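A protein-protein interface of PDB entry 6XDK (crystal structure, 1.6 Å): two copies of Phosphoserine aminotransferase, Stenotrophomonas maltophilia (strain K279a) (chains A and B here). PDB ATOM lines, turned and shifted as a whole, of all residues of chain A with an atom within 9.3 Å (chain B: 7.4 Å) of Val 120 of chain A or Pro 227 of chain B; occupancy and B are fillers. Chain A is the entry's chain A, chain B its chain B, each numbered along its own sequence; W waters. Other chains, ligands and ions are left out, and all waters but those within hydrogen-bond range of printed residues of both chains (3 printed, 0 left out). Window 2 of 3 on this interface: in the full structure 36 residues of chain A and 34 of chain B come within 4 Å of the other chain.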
ATOM      1  N   GLN A  88     -28.301 -14.102  21.559  1.00  0.00           N
ATOM      2  CA  GLN A  88     -27.426 -12.947  21.711  1.00  0.00           C
ATOM      3  C   GLN A  88     -26.007 -13.202  21.177  1.00  0.00           C
ATOM      4  O   GLN A  88     -25.296 -12.239  20.848  1.00  0.00           O
ATOM      5  CB  GLN A  88     -27.393 -12.527  23.186  1.00  0.00           C
ATOM      6  CG  GLN A  88     -28.685 -11.761  23.535  1.00  0.00           C
ATOM      7  CD  GLN A  88     -29.068 -11.769  25.001  1.00  0.00           C
ATOM      8  OE1 GLN A  88     -28.353 -12.282  25.850  1.00  0.00           O
ATOM      9  NE2 GLN A  88     -30.237 -11.176  25.300  1.00  0.00           N
ATOM     10  N   ALA A  89     -25.581 -14.460  21.075  1.00  0.00           N
ATOM     11  CA  ALA A  89     -24.326 -14.761  20.390  1.00  0.00           C
ATOM     12  C   ALA A  89     -24.547 -14.879  18.884  1.00  0.00           C
ATOM     13  O   ALA A  89     -23.705 -14.435  18.085  1.00  0.00           O
ATOM     14  CB  ALA A  89     -23.730 -16.067  20.944  1.00  0.00           C
ATOM     15  N   LEU A  90     -25.678 -15.481  18.490  1.00  0.00           N
ATOM     16  CA  LEU A  90     -25.937 -15.713  17.077  1.00  0.00           C
ATOM     17  C   LEU A  90     -26.243 -14.418  16.319  1.00  0.00           C
ATOM     18  O   LEU A  90     -25.922 -14.326  15.124  1.00  0.00           O
ATOM     19  CB  LEU A  90     -27.087 -16.725  16.928  1.00  0.00           C
ATOM     20  CG  LEU A  90     -26.735 -18.165  17.333  1.00  0.00           C
ATOM     21  CD1 LEU A  90     -27.913 -19.069  17.078  1.00  0.00           C
ATOM     22  CD2 LEU A  90     -25.530 -18.706  16.597  1.00  0.00           C
ATOM     23  N   PRO A  92     -24.828 -11.272  16.382  1.00  0.00           N
ATOM     24  CA  PRO A  92     -23.667 -10.674  15.711  1.00  0.00           C
ATOM     25  C   PRO A  92     -23.032 -11.618  14.705  1.00  0.00           C
ATOM     26  O   PRO A  92     -22.453 -11.157  13.719  1.00  0.00           O
ATOM     27  CB  PRO A  92     -22.705 -10.349  16.872  1.00  0.00           C
ATOM     28  CG  PRO A  92     -23.160 -11.244  17.984  1.00  0.00           C
ATOM     29  CD  PRO A  92     -24.641 -11.319  17.845  1.00  0.00           C
ATOM     30  N   LEU A  93     -23.117 -12.931  14.926  1.00  0.00           N
ATOM     31  CA  LEU A  93     -22.537 -13.881  13.965  1.00  0.00           C
ATOM     32  C   LEU A  93     -23.303 -13.902  12.650  1.00  0.00           C
ATOM     33  O   LEU A  93     -22.725 -14.212  11.599  1.00  0.00           O
ATOM     34  CB  LEU A  93     -22.525 -15.300  14.550  1.00  0.00           C
ATOM     35  CG  LEU A  93     -21.481 -15.555  15.643  1.00  0.00           C
ATOM     36  CD1 LEU A  93     -21.691 -16.935  16.248  1.00  0.00           C
ATOM     37  CD2 LEU A  93     -20.038 -15.321  15.155  1.00  0.00           C
ATOM     38  N   ALA A  97     -20.512  -8.165  10.032  1.00  0.00           N
ATOM     39  CA  ALA A  97     -19.223  -8.663   9.597  1.00  0.00           C
ATOM     40  C   ALA A  97     -18.295  -8.809  10.799  1.00  0.00           C
ATOM     41  O   ALA A  97     -18.493  -8.169  11.831  1.00  0.00           O
ATOM     42  CB  ALA A  97     -18.613  -7.722   8.571  1.00  0.00           C
ATOM     43  N   PRO A  98     -17.297  -9.689  10.717  1.00  0.00           N
ATOM     44  CA  PRO A  98     -16.363  -9.825  11.845  1.00  0.00           C
ATOM     45  C   PRO A  98     -15.778  -8.477  12.258  1.00  0.00           C
ATOM     46  O   PRO A  98     -15.262  -7.722  11.433  1.00  0.00           O
ATOM     47  CB  PRO A  98     -15.289 -10.766  11.296  1.00  0.00           C
ATOM     48  CG  PRO A  98     -16.029 -11.606  10.295  1.00  0.00           C
ATOM     49  CD  PRO A  98     -16.988 -10.631   9.625  1.00  0.00           C
ATOM     50  N   GLY A  99     -15.867  -8.184  13.552  1.00  0.00           N
ATOM     51  CA  GLY A  99     -15.318  -6.971  14.113  1.00  0.00           C
ATOM     52  C   GLY A  99     -16.054  -5.701  13.764  1.00  0.00           C
ATOM     53  O   GLY A  99     -15.579  -4.622  14.134  1.00  0.00           O
ATOM     54  N   GLN A 100     -17.169  -5.789  13.031  1.00  0.00           N
ATOM     55  CA  GLN A 100     -17.959  -4.599  12.726  1.00  0.00           C
ATOM     56  C   GLN A 100     -18.472  -3.960  14.004  1.00  0.00           C
ATOM     57  O   GLN A 100     -18.747  -4.628  14.992  1.00  0.00           O
ATOM     58  CB  GLN A 100     -19.143  -4.950  11.804  1.00  0.00           C
ATOM     59  CG  GLN A 100     -19.962  -3.740  11.358  1.00  0.00           C
ATOM     60  CD  GLN A 100     -21.005  -4.070  10.307  1.00  0.00           C
ATOM     61  OE1 GLN A 100     -21.184  -5.230   9.922  1.00  0.00           O
ATOM     62  NE2 GLN A 100     -21.685  -3.049   9.815  1.00  0.00           N
ATOM     63  N   TYR A 104     -25.103  -0.986  21.286  1.00  0.00           N
ATOM     64  CA  TYR A 104     -25.964  -1.565  22.307  1.00  0.00           C
ATOM     65  C   TYR A 104     -26.448  -0.478  23.246  1.00  0.00           C
ATOM     66  O   TYR A 104     -25.686   0.419  23.626  1.00  0.00           O
ATOM     67  CB  TYR A 104     -25.233  -2.651  23.126  1.00  0.00           C
ATOM     68  CG  TYR A 104     -25.180  -3.973  22.405  1.00  0.00           C
ATOM     69  CD1 TYR A 104     -24.332  -4.143  21.302  1.00  0.00           C
ATOM     70  CD2 TYR A 104     -25.987  -5.040  22.797  1.00  0.00           C
ATOM     71  CE1 TYR A 104     -24.279  -5.348  20.623  1.00  0.00           C
ATOM     72  CE2 TYR A 104     -25.954  -6.227  22.107  1.00  0.00           C
ATOM     73  CZ  TYR A 104     -25.101  -6.371  21.031  1.00  0.00           C
ATOM     74  OH  TYR A 104     -25.052  -7.553  20.341  1.00  0.00           O
ATOM     75  N   ALA A 114     -26.480  -9.394  26.942  1.00  0.00           N
ATOM     76  CA  ALA A 114     -26.390  -9.348  25.485  1.00  0.00           C
ATOM     77  C   ALA A 114     -25.035  -8.800  25.036  1.00  0.00           C
ATOM     78  O   ALA A 114     -24.416  -9.340  24.112  1.00  0.00           O
ATOM     79  CB  ALA A 114     -27.537  -8.507  24.917  1.00  0.00           C
ATOM     80  N   VAL A 115     -24.554  -7.737  25.688  1.00  0.00           N
ATOM     81  CA  VAL A 115     -23.229  -7.199  25.377  1.00  0.00           C
ATOM     82  C   VAL A 115     -22.162  -8.261  25.603  1.00  0.00           C
ATOM     83  O   VAL A 115     -21.239  -8.427  24.791  1.00  0.00           O
ATOM     84  CB  VAL A 115     -22.963  -5.946  26.226  1.00  0.00           C
ATOM     85  CG1 VAL A 115     -21.475  -5.551  26.152  1.00  0.00           C
ATOM     86  CG2 VAL A 115     -23.895  -4.797  25.786  1.00  0.00           C
ATOM     87  N   LYS A 116     -22.277  -8.996  26.712  1.00  0.00           N
ATOM     88  CA  LYS A 116     -21.276 -10.003  27.037  1.00  0.00           C
ATOM     89  C   LYS A 116     -21.152 -11.053  25.936  1.00  0.00           C
ATOM     90  O   LYS A 116     -20.027 -11.423  25.559  1.00  0.00           O
ATOM     91  CB  LYS A 116     -21.622 -10.667  28.363  1.00  0.00           C
ATOM     92  CG  LYS A 116     -20.551 -11.673  28.852  1.00  0.00           C
ATOM     93  CD  LYS A 116     -21.008 -12.345  30.123  1.00  0.00           C
ATOM     94  CE  LYS A 116     -19.977 -13.351  30.638  1.00  0.00           C
ATOM     95  NZ  LYS A 116     -20.494 -14.116  31.815  1.00  0.00           N
ATOM     96  N   GLN A 117     -22.289 -11.546  25.413  1.00  0.00           N
ATOM     97  CA  GLN A 117     -22.228 -12.595  24.388  1.00  0.00           C
ATOM     98  C   GLN A 117     -21.661 -12.068  23.082  1.00  0.00           C
ATOM     99  O   GLN A 117     -21.011 -12.813  22.341  1.00  0.00           O
ATOM    100  CB  GLN A 117     -23.611 -13.201  24.122  1.00  0.00           C
ATOM    101  CG  GLN A 117     -24.357 -13.755  25.349  1.00  0.00           C
ATOM    102  CD  GLN A 117     -23.497 -14.694  26.196  1.00  0.00           C
ATOM    103  OE1 GLN A 117     -22.742 -15.520  25.670  1.00  0.00           O
ATOM    104  NE2 GLN A 117     -23.596 -14.561  27.514  1.00  0.00           N
ATOM    105  N   ALA A 118     -21.873 -10.780  22.779  1.00  0.00           N
ATOM    106  CA  ALA A 118     -21.501 -10.245  21.477  1.00  0.00           C
ATOM    107  C   ALA A 118     -20.062  -9.754  21.402  1.00  0.00           C
ATOM    108  O   ALA A 118     -19.492  -9.706  20.304  1.00  0.00           O
ATOM    109  CB  ALA A 118     -22.460  -9.107  21.093  1.00  0.00           C
ATOM    110  N   GLY A 119     -19.431  -9.442  22.536  1.00  0.00           N
ATOM    111  CA  GLY A 119     -18.194  -8.680  22.509  1.00  0.00           C
ATOM    112  C   GLY A 119     -17.041  -9.369  21.814  1.00  0.00           C
ATOM    113  O   GLY A 119     -16.118  -8.695  21.338  1.00  0.00           O
ATOM    114  N   VAL A 120     -17.076 -10.695  21.727  1.00  0.00           N
ATOM    115  CA  VAL A 120     -16.011 -11.432  21.069  1.00  0.00           C
ATOM    116  C   VAL A 120     -16.125 -11.330  19.558  1.00  0.00           C
ATOM    117  O   VAL A 120     -15.118 -11.468  18.846  1.00  0.00           O
ATOM    118  CB  VAL A 120     -16.057 -12.894  21.581  1.00  0.00           C
ATOM    119  CG1 VAL A 120     -17.494 -13.445  21.556  1.00  0.00           C
ATOM    120  CG2 VAL A 120     -15.131 -13.785  20.801  1.00  0.00           C
ATOM    121  N   TYR A 121     -17.317 -11.028  19.052  1.00  0.00           N
ATOM    122  CA  TYR A 121     -17.592 -11.114  17.628  1.00  0.00           C
ATOM    123  C   TYR A 121     -17.702  -9.774  16.931  1.00  0.00           C
ATOM    124  O   TYR A 121     -17.478  -9.715  15.722  1.00  0.00           O
ATOM    125  CB  TYR A 121     -18.894 -11.874  17.396  1.00  0.00           C
ATOM    126  CG  TYR A 121     -18.898 -13.276  17.971  1.00  0.00           C
ATOM    127  CD1 TYR A 121     -17.874 -14.167  17.677  1.00  0.00           C
ATOM    128  CD2 TYR A 121     -19.914 -13.704  18.815  1.00  0.00           C
ATOM    129  CE1 TYR A 121     -17.874 -15.453  18.204  1.00  0.00           C
ATOM    130  CE2 TYR A 121     -19.931 -14.980  19.329  1.00  0.00           C
ATOM    131  CZ  TYR A 121     -18.903 -15.851  19.025  1.00  0.00           C
ATOM    132  OH  TYR A 121     -18.908 -17.126  19.537  1.00  0.00           O
ATOM    133  N   VAL A 122     -18.100  -8.717  17.654  1.00  0.00           N
ATOM    134  CA  VAL A 122     -18.289  -7.390  17.082  1.00  0.00           C
ATOM    135  C   VAL A 122     -17.626  -6.370  17.992  1.00  0.00           C
ATOM    136  O   VAL A 122     -17.342  -6.633  19.164  1.00  0.00           O
ATOM    137  CB  VAL A 122     -19.776  -7.034  16.893  1.00  0.00           C
ATOM    138  CG1 VAL A 122     -20.349  -7.839  15.754  1.00  0.00           C
ATOM    139  CG2 VAL A 122     -20.575  -7.287  18.172  1.00  0.00           C
ATOM    140  N   ASP A 123     -17.394  -5.184  17.437  1.00  0.00           N
ATOM    141  CA  ASP A 123     -16.878  -4.054  18.210  1.00  0.00           C
ATOM    142  C   ASP A 123     -18.075  -3.404  18.897  1.00  0.00           C
ATOM    143  O   ASP A 123     -18.775  -2.572  18.313  1.00  0.00           O
ATOM    144  CB  ASP A 123     -16.134  -3.082  17.299  1.00  0.00           C
ATOM    145  CG  ASP A 123     -15.657  -1.841  18.029  1.00  0.00           C
ATOM    146  OD1 ASP A 123     -15.466  -1.917  19.259  1.00  0.00           O
ATOM    147  OD2 ASP A 123     -15.523  -0.787  17.376  1.00  0.00           O
ATOM    148  N   VAL A 124     -18.348  -3.830  20.132  1.00  0.00           N
ATOM    149  CA  VAL A 124     -19.510  -3.327  20.859  1.00  0.00           C
ATOM    150  C   VAL A 124     -19.257  -1.891  21.267  1.00  0.00           C
ATOM    151  O   VAL A 124     -18.240  -1.582  21.897  1.00  0.00           O
ATOM    152  CB  VAL A 124     -19.804  -4.199  22.092  1.00  0.00           C
ATOM    153  CG1 VAL A 124     -20.918  -3.580  22.963  1.00  0.00           C
ATOM    154  CG2 VAL A 124     -20.146  -5.609  21.658  1.00  0.00           C
ATOM    155  N   TYR A 152     -26.137  -2.949  13.645  1.00  0.00           N
ATOM    156  CA  TYR A 152     -27.469  -2.918  14.219  1.00  0.00           C
ATOM    157  C   TYR A 152     -27.375  -2.110  15.504  1.00  0.00           C
ATOM    158  O   TYR A 152     -26.279  -1.830  16.002  1.00  0.00           O
ATOM    159  CB  TYR A 152     -28.004  -4.345  14.478  1.00  0.00           C
ATOM    160  CG  TYR A 152     -27.101  -5.235  15.319  1.00  0.00           C
ATOM    161  CD1 TYR A 152     -27.118  -5.142  16.710  1.00  0.00           C
ATOM    162  CD2 TYR A 152     -26.262  -6.170  14.728  1.00  0.00           C
ATOM    163  CE1 TYR A 152     -26.314  -5.957  17.498  1.00  0.00           C
ATOM    164  CE2 TYR A 152     -25.438  -6.983  15.482  1.00  0.00           C
ATOM    165  CZ  TYR A 152     -25.459  -6.875  16.871  1.00  0.00           C
ATOM    166  OH  TYR A 152     -24.674  -7.691  17.642  1.00  0.00           O
ATOM    167  N   GLN A 226     -20.698 -13.678   9.726  1.00  0.00           N
ATOM    168  CA  GLN A 226     -19.348 -14.159   9.966  1.00  0.00           C
ATOM    169  C   GLN A 226     -19.234 -15.647   9.670  1.00  0.00           C
ATOM    170  O   GLN A 226     -20.207 -16.378   9.832  1.00  0.00           O
ATOM    171  CB  GLN A 226     -18.962 -13.913  11.425  1.00  0.00           C
ATOM    172  CG  GLN A 226     -19.344 -12.505  11.864  1.00  0.00           C
ATOM    173  CD  GLN A 226     -18.696 -12.038  13.154  1.00  0.00           C
ATOM    174  OE1 GLN A 226     -17.703 -12.586  13.608  1.00  0.00           O
ATOM    175  NE2 GLN A 226     -19.259 -10.982  13.735  1.00  0.00           N
ATOM    176  N   PRO A 227     -18.066 -16.138   9.257  1.00  0.00           N
ATOM    177  CA  PRO A 227     -17.925 -17.575   8.995  1.00  0.00           C
ATOM    178  C   PRO A 227     -18.418 -18.385  10.188  1.00  0.00           C
ATOM    179  O   PRO A 227     -18.058 -18.117  11.341  1.00  0.00           O
ATOM    180  CB  PRO A 227     -16.415 -17.751   8.754  1.00  0.00           C
ATOM    181  CG  PRO A 227     -15.971 -16.363   8.251  1.00  0.00           C
ATOM    182  CD  PRO A 227     -16.821 -15.380   9.020  1.00  0.00           C
ATOM    183  N   PHE A 232     -25.414 -22.644  13.178  1.00  0.00           N
ATOM    184  CA  PHE A 232     -25.430 -21.288  13.708  1.00  0.00           C
ATOM    185  C   PHE A 232     -25.848 -20.268  12.654  1.00  0.00           C
ATOM    186  O   PHE A 232     -25.639 -19.065  12.840  1.00  0.00           O
ATOM    187  CB  PHE A 232     -24.049 -20.922  14.267  1.00  0.00           C
ATOM    188  CG  PHE A 232     -23.658 -21.689  15.505  1.00  0.00           C
ATOM    189  CD1 PHE A 232     -24.627 -22.274  16.323  1.00  0.00           C
ATOM    190  CD2 PHE A 232     -22.314 -21.805  15.857  1.00  0.00           C
ATOM    191  CE1 PHE A 232     -24.278 -22.967  17.460  1.00  0.00           C
ATOM    192  CE2 PHE A 232     -21.935 -22.533  17.023  1.00  0.00           C
ATOM    193  CZ  PHE A 232     -22.924 -23.097  17.822  1.00  0.00           C
ATOM    194  N   LEU B  93     -14.807 -25.671  18.686  1.00  0.00           N
ATOM    195  CA  LEU B  93     -14.608 -24.359  19.294  1.00  0.00           C
ATOM    196  C   LEU B  93     -14.120 -24.448  20.733  1.00  0.00           C
ATOM    197  O   LEU B  93     -13.504 -23.483  21.232  1.00  0.00           O
ATOM    198  CB  LEU B  93     -15.916 -23.563  19.297  1.00  0.00           C
ATOM    199  CG  LEU B  93     -16.336 -23.026  17.913  1.00  0.00           C
ATOM    200  CD1 LEU B  93     -17.791 -22.441  18.009  1.00  0.00           C
ATOM    201  CD2 LEU B  93     -15.341 -22.000  17.392  1.00  0.00           C
ATOM    202  N   ALA B  96     -10.240 -27.435  20.411  1.00  0.00           N
ATOM    203  CA  ALA B  96      -9.156 -27.275  19.455  1.00  0.00           C
ATOM    204  C   ALA B  96      -8.700 -25.829  19.401  1.00  0.00           C
ATOM    205  O   ALA B  96      -9.508 -24.908  19.550  1.00  0.00           O
ATOM    206  CB  ALA B  96      -9.607 -27.744  18.046  1.00  0.00           C
ATOM    207  N   ALA B  97      -7.402 -25.629  19.134  1.00  0.00           N
ATOM    208  CA  ALA B  97      -6.913 -24.293  18.796  1.00  0.00           C
ATOM    209  C   ALA B  97      -7.418 -23.894  17.409  1.00  0.00           C
ATOM    210  O   ALA B  97      -7.692 -24.750  16.583  1.00  0.00           O
ATOM    211  CB  ALA B  97      -5.392 -24.270  18.821  1.00  0.00           C
ATOM    212  N   PRO B  98      -7.566 -22.597  17.121  1.00  0.00           N
ATOM    213  CA  PRO B  98      -8.088 -22.205  15.798  1.00  0.00           C
ATOM    214  C   PRO B  98      -7.269 -22.800  14.650  1.00  0.00           C
ATOM    215  O   PRO B  98      -6.036 -22.740  14.643  1.00  0.00           O
ATOM    216  CB  PRO B  98      -8.006 -20.670  15.822  1.00  0.00           C
ATOM    217  CG  PRO B  98      -8.026 -20.313  17.301  1.00  0.00           C
ATOM    218  CD  PRO B  98      -7.277 -21.430  17.979  1.00  0.00           C
ATOM    219  N   TYR B 121     -14.091 -24.145  11.611  1.00  0.00           N
ATOM    220  CA  TYR B 121     -13.350 -23.840  12.826  1.00  0.00           C
ATOM    221  C   TYR B 121     -12.032 -24.566  12.970  1.00  0.00           C
ATOM    222  O   TYR B 121     -11.141 -24.069  13.664  1.00  0.00           O
ATOM    223  CB  TYR B 121     -14.196 -24.185  14.051  1.00  0.00           C
ATOM    224  CG  TYR B 121     -15.531 -23.481  14.065  1.00  0.00           C
ATOM    225  CD1 TYR B 121     -15.613 -22.095  13.880  1.00  0.00           C
ATOM    226  CD2 TYR B 121     -16.707 -24.194  14.249  1.00  0.00           C
ATOM    227  CE1 TYR B 121     -16.828 -21.448  13.898  1.00  0.00           C
ATOM    228  CE2 TYR B 121     -17.928 -23.559  14.278  1.00  0.00           C
ATOM    229  CZ  TYR B 121     -17.991 -22.181  14.098  1.00  0.00           C
ATOM    230  OH  TYR B 121     -19.193 -21.530  14.100  1.00  0.00           O
ATOM    231  N   SER B 224      -7.668 -24.063  25.781  1.00  0.00           N
ATOM    232  CA  SER B 224      -8.117 -22.705  25.463  1.00  0.00           C
ATOM    233  C   SER B 224      -9.298 -22.734  24.510  1.00  0.00           C
ATOM    234  O   SER B 224     -10.204 -21.895  24.608  1.00  0.00           O
ATOM    235  CB  SER B 224      -7.002 -21.896  24.808  1.00  0.00           C
ATOM    236  OG  SER B 224      -5.907 -21.713  25.685  1.00  0.00           O
ATOM    237  N   GLY B 225      -9.261 -23.647  23.547  1.00  0.00           N
ATOM    238  CA  GLY B 225     -10.254 -23.563  22.489  1.00  0.00           C
ATOM    239  C   GLY B 225     -10.051 -22.299  21.665  1.00  0.00           C
ATOM    240  O   GLY B 225      -8.936 -21.770  21.515  1.00  0.00           O
ATOM    241  N   GLN B 226     -11.159 -21.811  21.110  1.00  0.00           N
ATOM    242  CA  GLN B 226     -11.195 -20.705  20.170  1.00  0.00           C
ATOM    243  C   GLN B 226     -12.037 -19.565  20.717  1.00  0.00           C
ATOM    244  O   GLN B 226     -12.914 -19.797  21.545  1.00  0.00           O
ATOM    245  CB  GLN B 226     -11.793 -21.193  18.848  1.00  0.00           C
ATOM    246  CG  GLN B 226     -11.018 -22.405  18.358  1.00  0.00           C
ATOM    247  CD  GLN B 226     -11.290 -22.752  16.928  1.00  0.00           C
ATOM    248  OE1 GLN B 226     -11.560 -21.876  16.108  1.00  0.00           O
ATOM    249  NE2 GLN B 226     -11.171 -24.032  16.604  1.00  0.00           N
ATOM    250  N   PRO B 227     -11.794 -18.328  20.300  1.00  0.00           N
ATOM    251  CA  PRO B 227     -12.609 -17.220  20.816  1.00  0.00           C
ATOM    252  C   PRO B 227     -14.078 -17.519  20.593  1.00  0.00           C
ATOM    253  O   PRO B 227     -14.500 -17.908  19.497  1.00  0.00           O
ATOM    254  CB  PRO B 227     -12.135 -16.013  20.005  1.00  0.00           C
ATOM    255  CG  PRO B 227     -10.725 -16.379  19.613  1.00  0.00           C
ATOM    256  CD  PRO B 227     -10.677 -17.863  19.460  1.00  0.00           C
ATOM    257  N   ARG B 228     -14.861 -17.374  21.659  1.00  0.00           N
ATOM    258  CA  ARG B 228     -16.264 -17.754  21.581  1.00  0.00           C
ATOM    259  C   ARG B 228     -17.029 -17.085  22.708  1.00  0.00           C
ATOM    260  O   ARG B 228     -16.479 -16.816  23.777  1.00  0.00           O
ATOM    261  CB  ARG B 228     -16.422 -19.271  21.657  1.00  0.00           C
ATOM    262  CG  ARG B 228     -15.888 -19.889  22.961  1.00  0.00           C
ATOM    263  CD  ARG B 228     -15.676 -21.364  22.701  1.00  0.00           C
ATOM    264  NE  ARG B 228     -15.269 -22.101  23.899  1.00  0.00           N
ATOM    265  CZ  ARG B 228     -14.015 -22.151  24.363  1.00  0.00           C
ATOM    266  NH1 ARG B 228     -13.037 -21.426  23.796  1.00  0.00           N
ATOM    267  NH2 ARG B 228     -13.747 -22.905  25.430  1.00  0.00           N
ATOM    268  N   ALA B 229     -18.312 -16.815  22.446  1.00  0.00           N
ATOM    269  CA  ALA B 229     -19.199 -16.304  23.477  1.00  0.00           C
ATOM    270  C   ALA B 229     -19.299 -17.269  24.645  1.00  0.00           C
ATOM    271  O   ALA B 229     -19.166 -18.485  24.497  1.00  0.00           O
ATOM    272  CB  ALA B 229     -20.602 -16.069  22.899  1.00  0.00           C
ATOM    273  N   ASP B 230     -19.591 -16.700  25.813  1.00  0.00           N
ATOM    274  CA  ASP B 230     -19.702 -17.499  27.029  1.00  0.00           C
ATOM    275  C   ASP B 230     -20.732 -18.620  26.892  1.00  0.00           C
ATOM    276  O   ASP B 230     -20.536 -19.730  27.414  1.00  0.00           O
ATOM    277  CB  ASP B 230     -20.048 -16.557  28.185  1.00  0.00           C
ATOM    278  CG  ASP B 230     -19.867 -17.182  29.507  1.00  0.00           C
ATOM    279  OD1 ASP B 230     -18.703 -17.468  29.855  1.00  0.00           O
ATOM    280  OD2 ASP B 230     -20.889 -17.387  30.193  1.00  0.00           O
ATOM    281  N   PHE B 232     -21.330 -20.339  24.451  1.00  0.00           N
ATOM    282  CA  PHE B 232     -20.719 -21.399  23.663  1.00  0.00           C
ATOM    283  C   PHE B 232     -19.482 -22.003  24.339  1.00  0.00           C
ATOM    284  O   PHE B 232     -18.689 -22.705  23.678  1.00  0.00           O
ATOM    285  CB  PHE B 232     -20.361 -20.840  22.283  1.00  0.00           C
ATOM    286  CG  PHE B 232     -21.545 -20.516  21.416  1.00  0.00           C
ATOM    287  CD1 PHE B 232     -22.791 -21.079  21.639  1.00  0.00           C
ATOM    288  CD2 PHE B 232     -21.403 -19.612  20.364  1.00  0.00           C
ATOM    289  CE1 PHE B 232     -23.882 -20.725  20.804  1.00  0.00           C
ATOM    290  CE2 PHE B 232     -22.485 -19.285  19.538  1.00  0.00           C
ATOM    291  CZ  PHE B 232     -23.708 -19.858  19.763  1.00  0.00           C
HETATM  292  O   HOH W   1     -18.867 -18.905  14.324  1.00  0.00           O
HETATM  293  O   HOH W   2     -17.226 -18.709  18.315  1.00  0.00           O
HETATM  294  O   HOH W   3     -18.924 -13.942  26.145  1.00  0.00           O
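Water W2 lies within hydrogen-bond range of the side-chain hydroxyl (OH) of Tyr 121 of chain A and the backbone carbonyl oxygen (O) of Pro 227 of chain B.
Water W1 bridges OH of Tyr 121 of chain B and O of Pro 227 of chain A.
Water W3 lies within hydrogen-bond range of O of Lys 116 of chain A (2.8 Å) and N of Asp 230 of chain B (2.9 Å).
The backbone NH (N) of Gly 99 of chain A is in hydrogen-bond range of the backbone carbonyl oxygen (O) of Tyr 121 of chain A (3.1 Å).
The backbone carbonyl oxygen of Tyr 121 of chain A is in hydrogen-bond range of the side-chain amide nitrogen of Gln 226 of chain A (3.0 Å).
The guanidinium group (NH1) of Arg 228 of chain B sits at hydrogen-bond distance from the backbone carbonyl oxygen (O) of Leu 93 of chain B, at 3.3 Å.
NE2 of Gln 226 of chain B lies within hydrogen-bond range of O of Tyr 121 of chain B, 2.9 Å away.
The backbone carbonyl oxygen (O) of Ser 224 of chain B is in hydrogen-bond range of the guanidinium group (NH1) of Arg 228 of chain B (3.0 Å).
The guanidinium group (NE) of Arg 228 of chain B lies close to the backbone carbonyl oxygen (O) of Phe 232 of chain B (3.5 Å).
Among the printed residues, pairs that only touch across the chains: Gln 117 of chain A with Ala 229 of chain B (3.3 Å), Tyr 121 of chain A with Arg 228 of chain B (3.4 Å), Val 120 of chain A with Ala 229 of chain B (3.6 Å), Phe 232 of chain A with Tyr 121 of chain B (3.6 Å), Tyr 121 of chain A with Phe 232 of chain B (3.6 Å), Ala 89 of chain A with Ala 229 of chain B (3.7 Å), Val 120 of chain A with Arg 228 of chain B (3.7 Å), Ala 89 of chain A with Phe 232 of chain B (3.7 Å), Val 120 of chain A with Pro 227 of chain B (3.8 Å), Leu 90 of chain A with Phe 232 of chain B (3.8 Å) and Phe 232 of chain A with Phe 232 of chain B (3.9 Å).
Printed residues of chain B within 4 Å of Val 120 of chain A: Pro 227 (3.8 Å), Arg 228 (3.7 Å) and Ala 229 (3.6 Å).
Pro 227 of chain B touches one residue of chain A.
Printed residues of chain B within 4 Å of Lys 116 of chain A: Asp 230.
Of the printed residues of chain A, Asp 230 of chain B touches Lys 116 and Gln 117.
Of the printed residues of chain A, Tyr 121 of chain B touches Phe 232.
Of the printed residues of chain B, Leu 90 of chain A touches Phe 232 (3.8 Å).
Printed residues of chain B within 4 Å of Ala 89 of chain A: Ala 229 and Phe 232.
The nearest residue of chain A that does not touch Pro 227 of chain B is Tyr 121 of chain A (4.4 Å).
Of the 13 printed residues of chain B, 6 touch a printed residue of chain A.
Hydrophobic or aromatic side chains of chain B that line the printed part of chain A: Tyr 121, Pro 227, Ala 229 and Phe 232.
Printed residues of chain A that touch a printed residue of chain B: Ala 89, Leu 90, Lys 116, Gln 117, Val 120, Tyr 121 and Phe 232.
Hydrophobic or aromatic side chains of chain A that line the printed part of chain B: Ala 89, Leu 90, Val 120, Tyr 121 and Phe 232.
Among the printed residues, 14 pairs touch across the chains.
Among the printed residues, Asp or Glu carboxylates within 4 Å of a Lys or Arg side-chain nitrogen of the other chain: Lys 116 of chain A with Asp 230 of chain B.
Tyr 121 of chain A touches Phe 232 of chain B, and with the chains exchanged Phe 232 of chain A touches Tyr 121 of chain B.
Phe 232 of chain B touches its own counterpart, Phe 232 of chain A.
Positions printed for both chains: 93, 97, 98, 121, 226, 227 and 232.
OD2 of Asp 230 of chain B lies within salt-bridge range of NZ of Lys 116 of chain A, at 3.7 Å.
The side-chain amide oxygen (OE1) of Gln 117 of chain A is in hydrogen-bond range of the backbone NH (N) of Asp 230 of chain B, at 3.4 Å.
OH of Tyr 121 of chain A is in hydrogen-bond range of N of Ala 229 of chain B (3.0 Å).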
